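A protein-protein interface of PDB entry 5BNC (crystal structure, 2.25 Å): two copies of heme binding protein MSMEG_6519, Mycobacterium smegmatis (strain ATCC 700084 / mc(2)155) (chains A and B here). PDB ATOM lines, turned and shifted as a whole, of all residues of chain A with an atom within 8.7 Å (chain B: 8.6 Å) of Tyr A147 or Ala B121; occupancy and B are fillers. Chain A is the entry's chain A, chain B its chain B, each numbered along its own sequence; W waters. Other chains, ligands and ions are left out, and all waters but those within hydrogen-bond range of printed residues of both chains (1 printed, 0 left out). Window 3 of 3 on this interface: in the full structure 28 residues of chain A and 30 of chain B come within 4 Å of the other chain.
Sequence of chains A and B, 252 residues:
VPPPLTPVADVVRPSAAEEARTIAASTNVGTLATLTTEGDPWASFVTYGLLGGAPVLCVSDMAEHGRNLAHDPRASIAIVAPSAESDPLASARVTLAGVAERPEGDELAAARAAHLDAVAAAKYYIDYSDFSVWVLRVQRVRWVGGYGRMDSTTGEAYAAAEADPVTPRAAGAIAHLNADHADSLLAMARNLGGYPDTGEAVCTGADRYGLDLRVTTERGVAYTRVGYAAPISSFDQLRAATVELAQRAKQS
Of the printed residues of chain B, Asp A87 touches Ala B121 (3.7 Å).
Of the printed residues of chain B, Leu A89 touches Thr B47, Val B119 and Ala B121.
Trp A143 touches none of the printed residues of chain B.
Tyr A147 touches two residues of chain B.
Of the printed residues of chain A, Thr B47 touches Leu A89 (3.8 Å).
Printed residues of chain A within 4 Å of Val B119: Leu A89 (3.7 Å).
No residue of chain A comes within 4 Å of Ala B120.
Of the printed residues of chain A, Ala B121 touches Asp A87 (3.7 Å), Leu A89 (3.8 Å) and Tyr A147 (3.2 Å).
Printed residues of chain A within 4 Å of Tyr B125: Tyr A147 (3.6 Å).
The nearest residue of chain B that does not touch Tyr A147 is Tyr B124 (6.1 Å).
Of the 15 printed residues of chain B, 4 touch a printed residue of chain A.
Of the 17 printed residues of chain A, 3 touch a printed residue of chain B.
Hydrophobic or aromatic side chains of chain A within 4 Å of the printed part of chain B: Leu A89 and Tyr A147.
Along chain A the printed residues that touch a printed residue of chain B span positions 87 to 147.
Among the printed residues, 6 pairs touch across the chains.
Among the printed residues, no Asp or Glu carboxylate lies within 4 Å of a Lys or Arg side-chain nitrogen of the other chain.
No position is printed for both chains.
Of the 6 pairs that touch across the chains among the printed residues, none has its exchanged pair printed and touching as well.
Water W1 lies within hydrogen-bond range of N of Ala B121 (2.8 Å), N of Ala B120 (3.0 Å) and OD1 of Asp A87 (3.3 Å).
The side-chain carboxylate (OD2) of Asp A87 sits at hydrogen-bond distance from the side-chain hydroxyl (OH) of Tyr A147 (2.4 Å).
N of Leu A89 lies close to OD1 of Asp A87 (3.2 Å).
The backbone carbonyl oxygen of Leu A89 is in hydrogen-bond range of the guanidinium group of Arg A93 (2.9 Å).
Among the printed residues, merely in contact across the chains: Tyr A147 with Ala B121 (3.2 Å), Tyr A147 with Tyr B125 (3.6 Å), Asp A87 with Ala B121 (3.7 Å), Leu A89 with Val B119 (3.7 Å), Leu A89 with Ala B121 (3.8 Å) and Leu A89 with Thr B47 (3.8 Å).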
ATOM      1  N   GLU A  85     -24.856  20.384 -10.292  1.00  0.00           N
ATOM      2  CA  GLU A  85     -24.391  20.230 -11.682  1.00  0.00           C
ATOM      3  C   GLU A  85     -22.910  20.058 -11.806  1.00  0.00           C
ATOM      4  O   GLU A  85     -22.152  20.761 -11.177  1.00  0.00           O
ATOM      5  CB  GLU A  85     -24.797  21.425 -12.560  1.00  0.00           C
ATOM      6  CG  GLU A  85     -26.074  21.175 -13.340  1.00  0.00           C
ATOM      7  CD  GLU A  85     -26.768  22.452 -13.700  1.00  0.00           C
ATOM      8  OE1 GLU A  85     -26.487  23.472 -13.038  1.00  0.00           O
ATOM      9  OE2 GLU A  85     -27.577  22.437 -14.646  1.00  0.00           O
ATOM     10  N   SER A  86     -22.519  19.106 -12.632  1.00  0.00           N
ATOM     11  CA  SER A  86     -21.126  18.839 -12.875  1.00  0.00           C
ATOM     12  C   SER A  86     -20.614  19.631 -14.077  1.00  0.00           C
ATOM     13  O   SER A  86     -19.465  19.510 -14.412  1.00  0.00           O
ATOM     14  CB  SER A  86     -20.963  17.352 -13.155  1.00  0.00           C
ATOM     15  OG  SER A  86     -21.663  17.029 -14.351  1.00  0.00           O
ATOM     16  N   ASP A  87     -21.478  20.370 -14.766  1.00  0.00           N
ATOM     17  CA  ASP A  87     -21.031  21.225 -15.848  1.00  0.00           C
ATOM     18  C   ASP A  87     -20.680  22.599 -15.247  1.00  0.00           C
ATOM     19  O   ASP A  87     -21.586  23.351 -14.866  1.00  0.00           O
ATOM     20  CB  ASP A  87     -22.105  21.405 -16.912  1.00  0.00           C
ATOM     21  CG  ASP A  87     -21.651  22.332 -18.040  1.00  0.00           C
ATOM     22  OD1 ASP A  87     -20.433  22.691 -18.076  1.00  0.00           O
ATOM     23  OD2 ASP A  87     -22.518  22.675 -18.904  1.00  0.00           O
ATOM     24  N   PRO A  88     -19.374  22.915 -15.148  1.00  0.00           N
ATOM     25  CA  PRO A  88     -18.938  24.150 -14.492  1.00  0.00           C
ATOM     26  C   PRO A  88     -19.556  25.415 -15.114  1.00  0.00           C
ATOM     27  O   PRO A  88     -19.834  26.372 -14.418  1.00  0.00           O
ATOM     28  CB  PRO A  88     -17.411  24.139 -14.639  1.00  0.00           C
ATOM     29  CG  PRO A  88     -17.036  22.861 -15.323  1.00  0.00           C
ATOM     30  CD  PRO A  88     -18.266  22.117 -15.709  1.00  0.00           C
ATOM     31  N   LEU A  89     -19.822  25.382 -16.410  1.00  0.00           N
ATOM     32  CA  LEU A  89     -20.357  26.541 -17.092  1.00  0.00           C
ATOM     33  C   LEU A  89     -21.754  26.870 -16.647  1.00  0.00           C
ATOM     34  O   LEU A  89     -22.243  27.968 -16.904  1.00  0.00           O
ATOM     35  CB  LEU A  89     -20.342  26.338 -18.603  1.00  0.00           C
ATOM     36  CG  LEU A  89     -18.995  26.382 -19.320  1.00  0.00           C
ATOM     37  CD1 LEU A  89     -18.055  27.460 -18.803  1.00  0.00           C
ATOM     38  CD2 LEU A  89     -18.303  25.048 -19.233  1.00  0.00           C
ATOM     39  N   ALA A  90     -22.416  25.900 -16.025  1.00  0.00           N
ATOM     40  CA  ALA A  90     -23.748  26.108 -15.436  1.00  0.00           C
ATOM     41  C   ALA A  90     -23.684  26.786 -14.076  1.00  0.00           C
ATOM     42  O   ALA A  90     -24.712  27.178 -13.523  1.00  0.00           O
ATOM     43  CB  ALA A  90     -24.475  24.783 -15.289  1.00  0.00           C
ATOM     44  N   SER A  91     -22.480  26.899 -13.523  1.00  0.00           N
ATOM     45  CA  SER A  91     -22.290  27.545 -12.242  1.00  0.00           C
ATOM     46  C   SER A  91     -22.858  28.963 -12.208  1.00  0.00           C
ATOM     47  O   SER A  91     -22.787  29.688 -13.165  1.00  0.00           O
ATOM     48  CB  SER A  91     -20.803  27.644 -11.931  1.00  0.00           C
ATOM     49  OG  SER A  91     -20.264  26.389 -11.663  1.00  0.00           O
ATOM     50  N   ALA A  92     -23.402  29.345 -11.071  1.00  0.00           N
ATOM     51  CA  ALA A  92     -23.680  30.746 -10.783  1.00  0.00           C
ATOM     52  C   ALA A  92     -22.452  31.404 -10.087  1.00  0.00           C
ATOM     53  O   ALA A  92     -21.999  30.884  -9.045  1.00  0.00           O
ATOM     54  CB  ALA A  92     -24.913  30.852  -9.881  1.00  0.00           C
ATOM     55  N   ARG A  93     -21.974  32.552 -10.616  1.00  0.00           N
ATOM     56  CA  ARG A  93     -20.772  33.236 -10.103  1.00  0.00           C
ATOM     57  C   ARG A  93     -20.955  34.721 -10.121  1.00  0.00           C
ATOM     58  O   ARG A  93     -21.759  35.259 -10.928  1.00  0.00           O
ATOM     59  CB  ARG A  93     -19.438  33.020 -10.924  1.00  0.00           C
ATOM     60  CG  ARG A  93     -19.397  32.075 -12.115  1.00  0.00           C
ATOM     61  CD  ARG A  93     -20.483  32.138 -13.147  1.00  0.00           C
ATOM     62  NE  ARG A  93     -19.968  32.062 -14.503  1.00  0.00           N
ATOM     63  CZ  ARG A  93     -20.245  31.160 -15.435  1.00  0.00           C
ATOM     64  NH1 ARG A  93     -19.637  31.291 -16.579  1.00  0.00           N
ATOM     65  NH2 ARG A  93     -21.086  30.126 -15.294  1.00  0.00           N
ATOM     66  N   TRP A 143     -22.493  39.759 -12.508  1.00  0.00           N
ATOM     67  CA  TRP A 143     -23.108  38.472 -12.185  1.00  0.00           C
ATOM     68  C   TRP A 143     -23.352  37.649 -13.439  1.00  0.00           C
ATOM     69  O   TRP A 143     -23.809  38.177 -14.454  1.00  0.00           O
ATOM     70  CB  TRP A 143     -24.412  38.705 -11.442  1.00  0.00           C
ATOM     71  CG  TRP A 143     -25.347  37.554 -11.422  1.00  0.00           C
ATOM     72  CD1 TRP A 143     -25.224  36.417 -10.701  1.00  0.00           C
ATOM     73  CD2 TRP A 143     -26.584  37.439 -12.157  1.00  0.00           C
ATOM     74  NE1 TRP A 143     -26.305  35.573 -10.944  1.00  0.00           N
ATOM     75  CE2 TRP A 143     -27.154  36.177 -11.828  1.00  0.00           C
ATOM     76  CE3 TRP A 143     -27.260  38.275 -13.058  1.00  0.00           C
ATOM     77  CZ2 TRP A 143     -28.393  35.744 -12.331  1.00  0.00           C
ATOM     78  CZ3 TRP A 143     -28.513  37.836 -13.578  1.00  0.00           C
ATOM     79  CH2 TRP A 143     -29.049  36.575 -13.205  1.00  0.00           C
ATOM     80  N   VAL A 144     -22.953  36.384 -13.374  1.00  0.00           N
ATOM     81  CA  VAL A 144     -23.233  35.397 -14.416  1.00  0.00           C
ATOM     82  C   VAL A 144     -23.945  34.225 -13.793  1.00  0.00           C
ATOM     83  O   VAL A 144     -23.326  33.428 -13.062  1.00  0.00           O
ATOM     84  CB  VAL A 144     -21.979  34.915 -15.102  1.00  0.00           C
ATOM     85  CG1 VAL A 144     -22.304  33.914 -16.182  1.00  0.00           C
ATOM     86  CG2 VAL A 144     -21.299  36.085 -15.764  1.00  0.00           C
ATOM     87  N   GLY A 145     -25.259  34.160 -14.042  1.00  0.00           N
ATOM     88  CA  GLY A 145     -26.104  33.074 -13.557  1.00  0.00           C
ATOM     89  C   GLY A 145     -26.107  31.894 -14.527  1.00  0.00           C
ATOM     90  O   GLY A 145     -27.073  31.657 -15.233  1.00  0.00           O
ATOM     91  N   GLY A 146     -25.030  31.134 -14.538  1.00  0.00           N
ATOM     92  CA  GLY A 146     -24.963  29.929 -15.328  1.00  0.00           C
ATOM     93  C   GLY A 146     -25.073  30.199 -16.812  1.00  0.00           C
ATOM     94  O   GLY A 146     -24.567  31.196 -17.328  1.00  0.00           O
ATOM     95  N   TYR A 147     -25.786  29.315 -17.498  1.00  0.00           N
ATOM     96  CA  TYR A 147     -26.094  29.542 -18.887  1.00  0.00           C
ATOM     97  C   TYR A 147     -27.122  30.674 -19.020  1.00  0.00           C
ATOM     98  O   TYR A 147     -27.162  31.331 -20.048  1.00  0.00           O
ATOM     99  CB  TYR A 147     -26.566  28.244 -19.534  1.00  0.00           C
ATOM    100  CG  TYR A 147     -25.440  27.241 -19.782  1.00  0.00           C
ATOM    101  CD1 TYR A 147     -24.496  27.457 -20.783  1.00  0.00           C
ATOM    102  CD2 TYR A 147     -25.323  26.090 -19.010  1.00  0.00           C
ATOM    103  CE1 TYR A 147     -23.464  26.554 -21.006  1.00  0.00           C
ATOM    104  CE2 TYR A 147     -24.301  25.180 -19.237  1.00  0.00           C
ATOM    105  CZ  TYR A 147     -23.380  25.413 -20.245  1.00  0.00           C
ATOM    106  OH  TYR A 147     -22.373  24.513 -20.496  1.00  0.00           O
ATOM    107  N   GLY A 148     -27.878  30.940 -17.950  1.00  0.00           N
ATOM    108  CA  GLY A 148     -28.949  31.939 -17.969  1.00  0.00           C
ATOM    109  C   GLY A 148     -28.583  33.423 -18.128  1.00  0.00           C
ATOM    110  O   GLY A 148     -27.815  33.824 -19.019  1.00  0.00           O
ATOM    111  N   ARG A 149     -29.155  34.263 -17.276  1.00  0.00           N
ATOM    112  CA  ARG A 149     -28.924  35.688 -17.440  1.00  0.00           C
ATOM    113  C   ARG A 149     -27.488  36.080 -16.968  1.00  0.00           C
ATOM    114  O   ARG A 149     -26.816  35.344 -16.258  1.00  0.00           O
ATOM    115  CB  ARG A 149     -30.028  36.499 -16.732  1.00  0.00           C
ATOM    116  N   MET A 150     -27.017  37.220 -17.444  1.00  0.00           N
ATOM    117  CA  MET A 150     -25.872  37.892 -16.851  1.00  0.00           C
ATOM    118  C   MET A 150     -26.172  39.370 -16.799  1.00  0.00           C
ATOM    119  O   MET A 150     -26.972  39.863 -17.566  1.00  0.00           O
ATOM    120  CB  MET A 150     -24.582  37.659 -17.626  1.00  0.00           C
ATOM    121  CG  MET A 150     -24.588  38.227 -19.011  1.00  0.00           C
ATOM    122  SD  MET A 150     -23.278  37.375 -19.917  1.00  0.00           S
ATOM    123  CE  MET A 150     -23.785  37.641 -21.619  1.00  0.00           C
ATOM    124  N   ASN B  28     -10.636  21.523 -13.390  1.00  0.00           N
ATOM    125  CA  ASN B  28     -10.701  22.346 -14.612  1.00  0.00           C
ATOM    126  C   ASN B  28     -11.325  23.744 -14.404  1.00  0.00           C
ATOM    127  O   ASN B  28     -11.766  24.402 -15.365  1.00  0.00           O
ATOM    128  CB  ASN B  28     -11.475  21.594 -15.658  1.00  0.00           C
ATOM    129  CG  ASN B  28     -12.912  21.340 -15.249  1.00  0.00           C
ATOM    130  OD1 ASN B  28     -13.361  21.606 -14.119  1.00  0.00           O
ATOM    131  ND2 ASN B  28     -13.670  20.842 -16.201  1.00  0.00           N
ATOM    132  N   THR B  47     -12.749  28.278 -16.765  1.00  0.00           N
ATOM    133  CA  THR B  47     -12.481  26.875 -16.973  1.00  0.00           C
ATOM    134  C   THR B  47     -11.214  26.729 -17.766  1.00  0.00           C
ATOM    135  O   THR B  47     -10.843  27.632 -18.513  1.00  0.00           O
ATOM    136  CB  THR B  47     -13.622  26.209 -17.738  1.00  0.00           C
ATOM    137  OG1 THR B  47     -13.873  26.912 -18.937  1.00  0.00           O
ATOM    138  CG2 THR B  47     -14.906  26.277 -16.945  1.00  0.00           C
ATOM    139  N   CYS B  58     -10.564  29.388 -22.840  1.00  0.00           N
ATOM    140  CA  CYS B  58     -11.330  29.761 -24.004  1.00  0.00           C
ATOM    141  C   CYS B  58     -12.208  30.904 -23.547  1.00  0.00           C
ATOM    142  O   CYS B  58     -13.148  30.701 -22.780  1.00  0.00           O
ATOM    143  CB  CYS B  58     -12.188  28.585 -24.472  1.00  0.00           C
ATOM    144  SG  CYS B  58     -13.318  28.984 -25.854  1.00  0.00           S
ATOM    145  N   HIS B 115      -8.116  21.903 -24.162  1.00  0.00           N
ATOM    146  CA  HIS B 115      -9.234  22.581 -23.514  1.00  0.00           C
ATOM    147  C   HIS B 115     -10.488  21.768 -23.685  1.00  0.00           C
ATOM    148  O   HIS B 115     -11.220  21.541 -22.731  1.00  0.00           O
ATOM    149  CB  HIS B 115      -9.439  24.000 -24.103  1.00  0.00           C
ATOM    150  CG  HIS B 115     -10.460  24.805 -23.370  1.00  0.00           C
ATOM    151  ND1 HIS B 115     -10.138  25.645 -22.327  1.00  0.00           N
ATOM    152  CD2 HIS B 115     -11.807  24.828 -23.469  1.00  0.00           C
ATOM    153  CE1 HIS B 115     -11.239  26.170 -21.836  1.00  0.00           C
ATOM    154  NE2 HIS B 115     -12.265  25.717 -22.531  1.00  0.00           N
ATOM    155  N   LEU B 116     -10.770  21.394 -24.931  1.00  0.00           N
ATOM    156  CA  LEU B 116     -11.931  20.568 -25.252  1.00  0.00           C
ATOM    157  C   LEU B 116     -12.046  19.283 -24.475  1.00  0.00           C
ATOM    158  O   LEU B 116     -13.121  18.897 -24.107  1.00  0.00           O
ATOM    159  CB  LEU B 116     -11.914  20.183 -26.717  1.00  0.00           C
ATOM    160  CG  LEU B 116     -12.491  21.226 -27.651  1.00  0.00           C
ATOM    161  CD1 LEU B 116     -12.301  20.751 -29.080  1.00  0.00           C
ATOM    162  CD2 LEU B 116     -13.961  21.459 -27.339  1.00  0.00           C
ATOM    163  N   ASP B 117     -10.959  18.588 -24.228  1.00  0.00           N
ATOM    164  CA  ASP B 117     -11.151  17.327 -23.508  1.00  0.00           C
ATOM    165  C   ASP B 117     -11.163  17.498 -22.008  1.00  0.00           C
ATOM    166  O   ASP B 117     -11.562  16.578 -21.311  1.00  0.00           O
ATOM    167  CB  ASP B 117     -10.241  16.160 -23.972  1.00  0.00           C
ATOM    168  CG  ASP B 117      -8.789  16.478 -23.884  1.00  0.00           C
ATOM    169  OD1 ASP B 117      -8.451  17.543 -23.313  1.00  0.00           O
ATOM    170  OD2 ASP B 117      -7.980  15.658 -24.393  1.00  0.00           O
ATOM    171  N   ALA B 118     -10.813  18.683 -21.503  1.00  0.00           N
ATOM    172  CA  ALA B 118     -10.989  18.989 -20.069  1.00  0.00           C
ATOM    173  C   ALA B 118     -12.331  19.647 -19.745  1.00  0.00           C
ATOM    174  O   ALA B 118     -12.772  19.608 -18.611  1.00  0.00           O
ATOM    175  CB  ALA B 118      -9.863  19.870 -19.603  1.00  0.00           C
ATOM    176  N   VAL B 119     -12.971  20.256 -20.744  1.00  0.00           N
ATOM    177  CA  VAL B 119     -14.223  20.986 -20.533  1.00  0.00           C
ATOM    178  C   VAL B 119     -15.193  20.640 -21.663  1.00  0.00           C
ATOM    179  O   VAL B 119     -15.167  21.235 -22.759  1.00  0.00           O
ATOM    180  CB  VAL B 119     -13.980  22.505 -20.524  1.00  0.00           C
ATOM    181  CG1 VAL B 119     -15.223  23.224 -20.033  1.00  0.00           C
ATOM    182  CG2 VAL B 119     -12.771  22.848 -19.692  1.00  0.00           C
ATOM    183  N   ALA B 120     -16.053  19.674 -21.393  1.00  0.00           N
ATOM    184  CA  ALA B 120     -16.881  19.082 -22.431  1.00  0.00           C
ATOM    185  C   ALA B 120     -17.722  20.167 -23.105  1.00  0.00           C
ATOM    186  O   ALA B 120     -17.829  20.199 -24.333  1.00  0.00           O
ATOM    187  CB  ALA B 120     -17.753  17.997 -21.824  1.00  0.00           C
ATOM    188  N   ALA B 121     -18.276  21.081 -22.307  1.00  0.00           N
ATOM    189  CA  ALA B 121     -19.203  22.066 -22.834  1.00  0.00           C
ATOM    190  C   ALA B 121     -18.555  23.111 -23.734  1.00  0.00           C
ATOM    191  O   ALA B 121     -19.246  23.815 -24.453  1.00  0.00           O
ATOM    192  CB  ALA B 121     -19.991  22.728 -21.709  1.00  0.00           C
ATOM    193  N   ALA B 122     -17.233  23.209 -23.717  1.00  0.00           N
ATOM    194  CA  ALA B 122     -16.547  24.184 -24.552  1.00  0.00           C
ATOM    195  C   ALA B 122     -16.740  23.841 -26.054  1.00  0.00           C
ATOM    196  O   ALA B 122     -16.504  24.681 -26.935  1.00  0.00           O
ATOM    197  CB  ALA B 122     -15.071  24.241 -24.176  1.00  0.00           C
ATOM    198  N   LYS B 123     -17.098  22.583 -26.302  1.00  0.00           N
ATOM    199  CA  LYS B 123     -17.663  22.112 -27.562  1.00  0.00           C
ATOM    200  C   LYS B 123     -18.485  23.211 -28.251  1.00  0.00           C
ATOM    201  O   LYS B 123     -18.256  23.496 -29.414  1.00  0.00           O
ATOM    202  CB  LYS B 123     -18.500  20.872 -27.229  1.00  0.00           C
ATOM    203  CG  LYS B 123     -19.398  20.252 -28.298  1.00  0.00           C
ATOM    204  CD  LYS B 123     -20.209  19.090 -27.680  1.00  0.00           C
ATOM    205  CE  LYS B 123     -21.544  18.808 -28.383  1.00  0.00           C
ATOM    206  NZ  LYS B 123     -21.534  17.632 -29.296  1.00  0.00           N
ATOM    207  N   TYR B 124     -19.356  23.890 -27.496  1.00  0.00           N
ATOM    208  CA  TYR B 124     -20.351  24.812 -28.058  1.00  0.00           C
ATOM    209  C   TYR B 124     -19.824  26.225 -28.327  1.00  0.00           C
ATOM    210  O   TYR B 124     -20.533  27.024 -28.937  1.00  0.00           O
ATOM    211  CB  TYR B 124     -21.596  24.933 -27.148  1.00  0.00           C
ATOM    212  CG  TYR B 124     -22.323  23.643 -26.790  1.00  0.00           C
ATOM    213  CD1 TYR B 124     -21.634  22.559 -26.265  1.00  0.00           C
ATOM    214  CD2 TYR B 124     -23.715  23.528 -26.916  1.00  0.00           C
ATOM    215  CE1 TYR B 124     -22.279  21.384 -25.906  1.00  0.00           C
ATOM    216  CE2 TYR B 124     -24.375  22.348 -26.553  1.00  0.00           C
ATOM    217  CZ  TYR B 124     -23.644  21.278 -26.046  1.00  0.00           C
ATOM    218  OH  TYR B 124     -24.228  20.090 -25.666  1.00  0.00           O
ATOM    219  N   TYR B 125     -18.588  26.528 -27.911  1.00  0.00           N
ATOM    220  CA  TYR B 125     -18.039  27.907 -27.985  1.00  0.00           C
ATOM    221  C   TYR B 125     -16.780  28.053 -28.793  1.00  0.00           C
ATOM    222  O   TYR B 125     -16.529  29.124 -29.341  1.00  0.00           O
ATOM    223  CB  TYR B 125     -17.743  28.441 -26.566  1.00  0.00           C
ATOM    224  CG  TYR B 125     -19.011  28.563 -25.764  1.00  0.00           C
ATOM    225  CD1 TYR B 125     -19.920  29.622 -25.992  1.00  0.00           C
ATOM    226  CD2 TYR B 125     -19.367  27.601 -24.822  1.00  0.00           C
ATOM    227  CE1 TYR B 125     -21.127  29.731 -25.276  1.00  0.00           C
ATOM    228  CE2 TYR B 125     -20.571  27.707 -24.107  1.00  0.00           C
ATOM    229  CZ  TYR B 125     -21.445  28.769 -24.340  1.00  0.00           C
ATOM    230  OH  TYR B 125     -22.614  28.857 -23.623  1.00  0.00           O
ATOM    231  N   ILE B 126     -15.938  27.023 -28.812  1.00  0.00           N
ATOM    232  CA  ILE B 126     -14.517  27.245 -29.092  1.00  0.00           C
ATOM    233  C   ILE B 126     -14.262  27.573 -30.553  1.00  0.00           C
ATOM    234  O   ILE B 126     -13.227  28.178 -30.886  1.00  0.00           O
ATOM    235  CB  ILE B 126     -13.615  26.086 -28.543  1.00  0.00           C
ATOM    236  CG1 ILE B 126     -12.147  26.515 -28.417  1.00  0.00           C
ATOM    237  CG2 ILE B 126     -13.740  24.824 -29.376  1.00  0.00           C
ATOM    238  CD1 ILE B 126     -11.323  25.554 -27.583  1.00  0.00           C
HETATM  239  O   HOH W   1     -18.185  20.720 -19.571  1.00  0.00           O
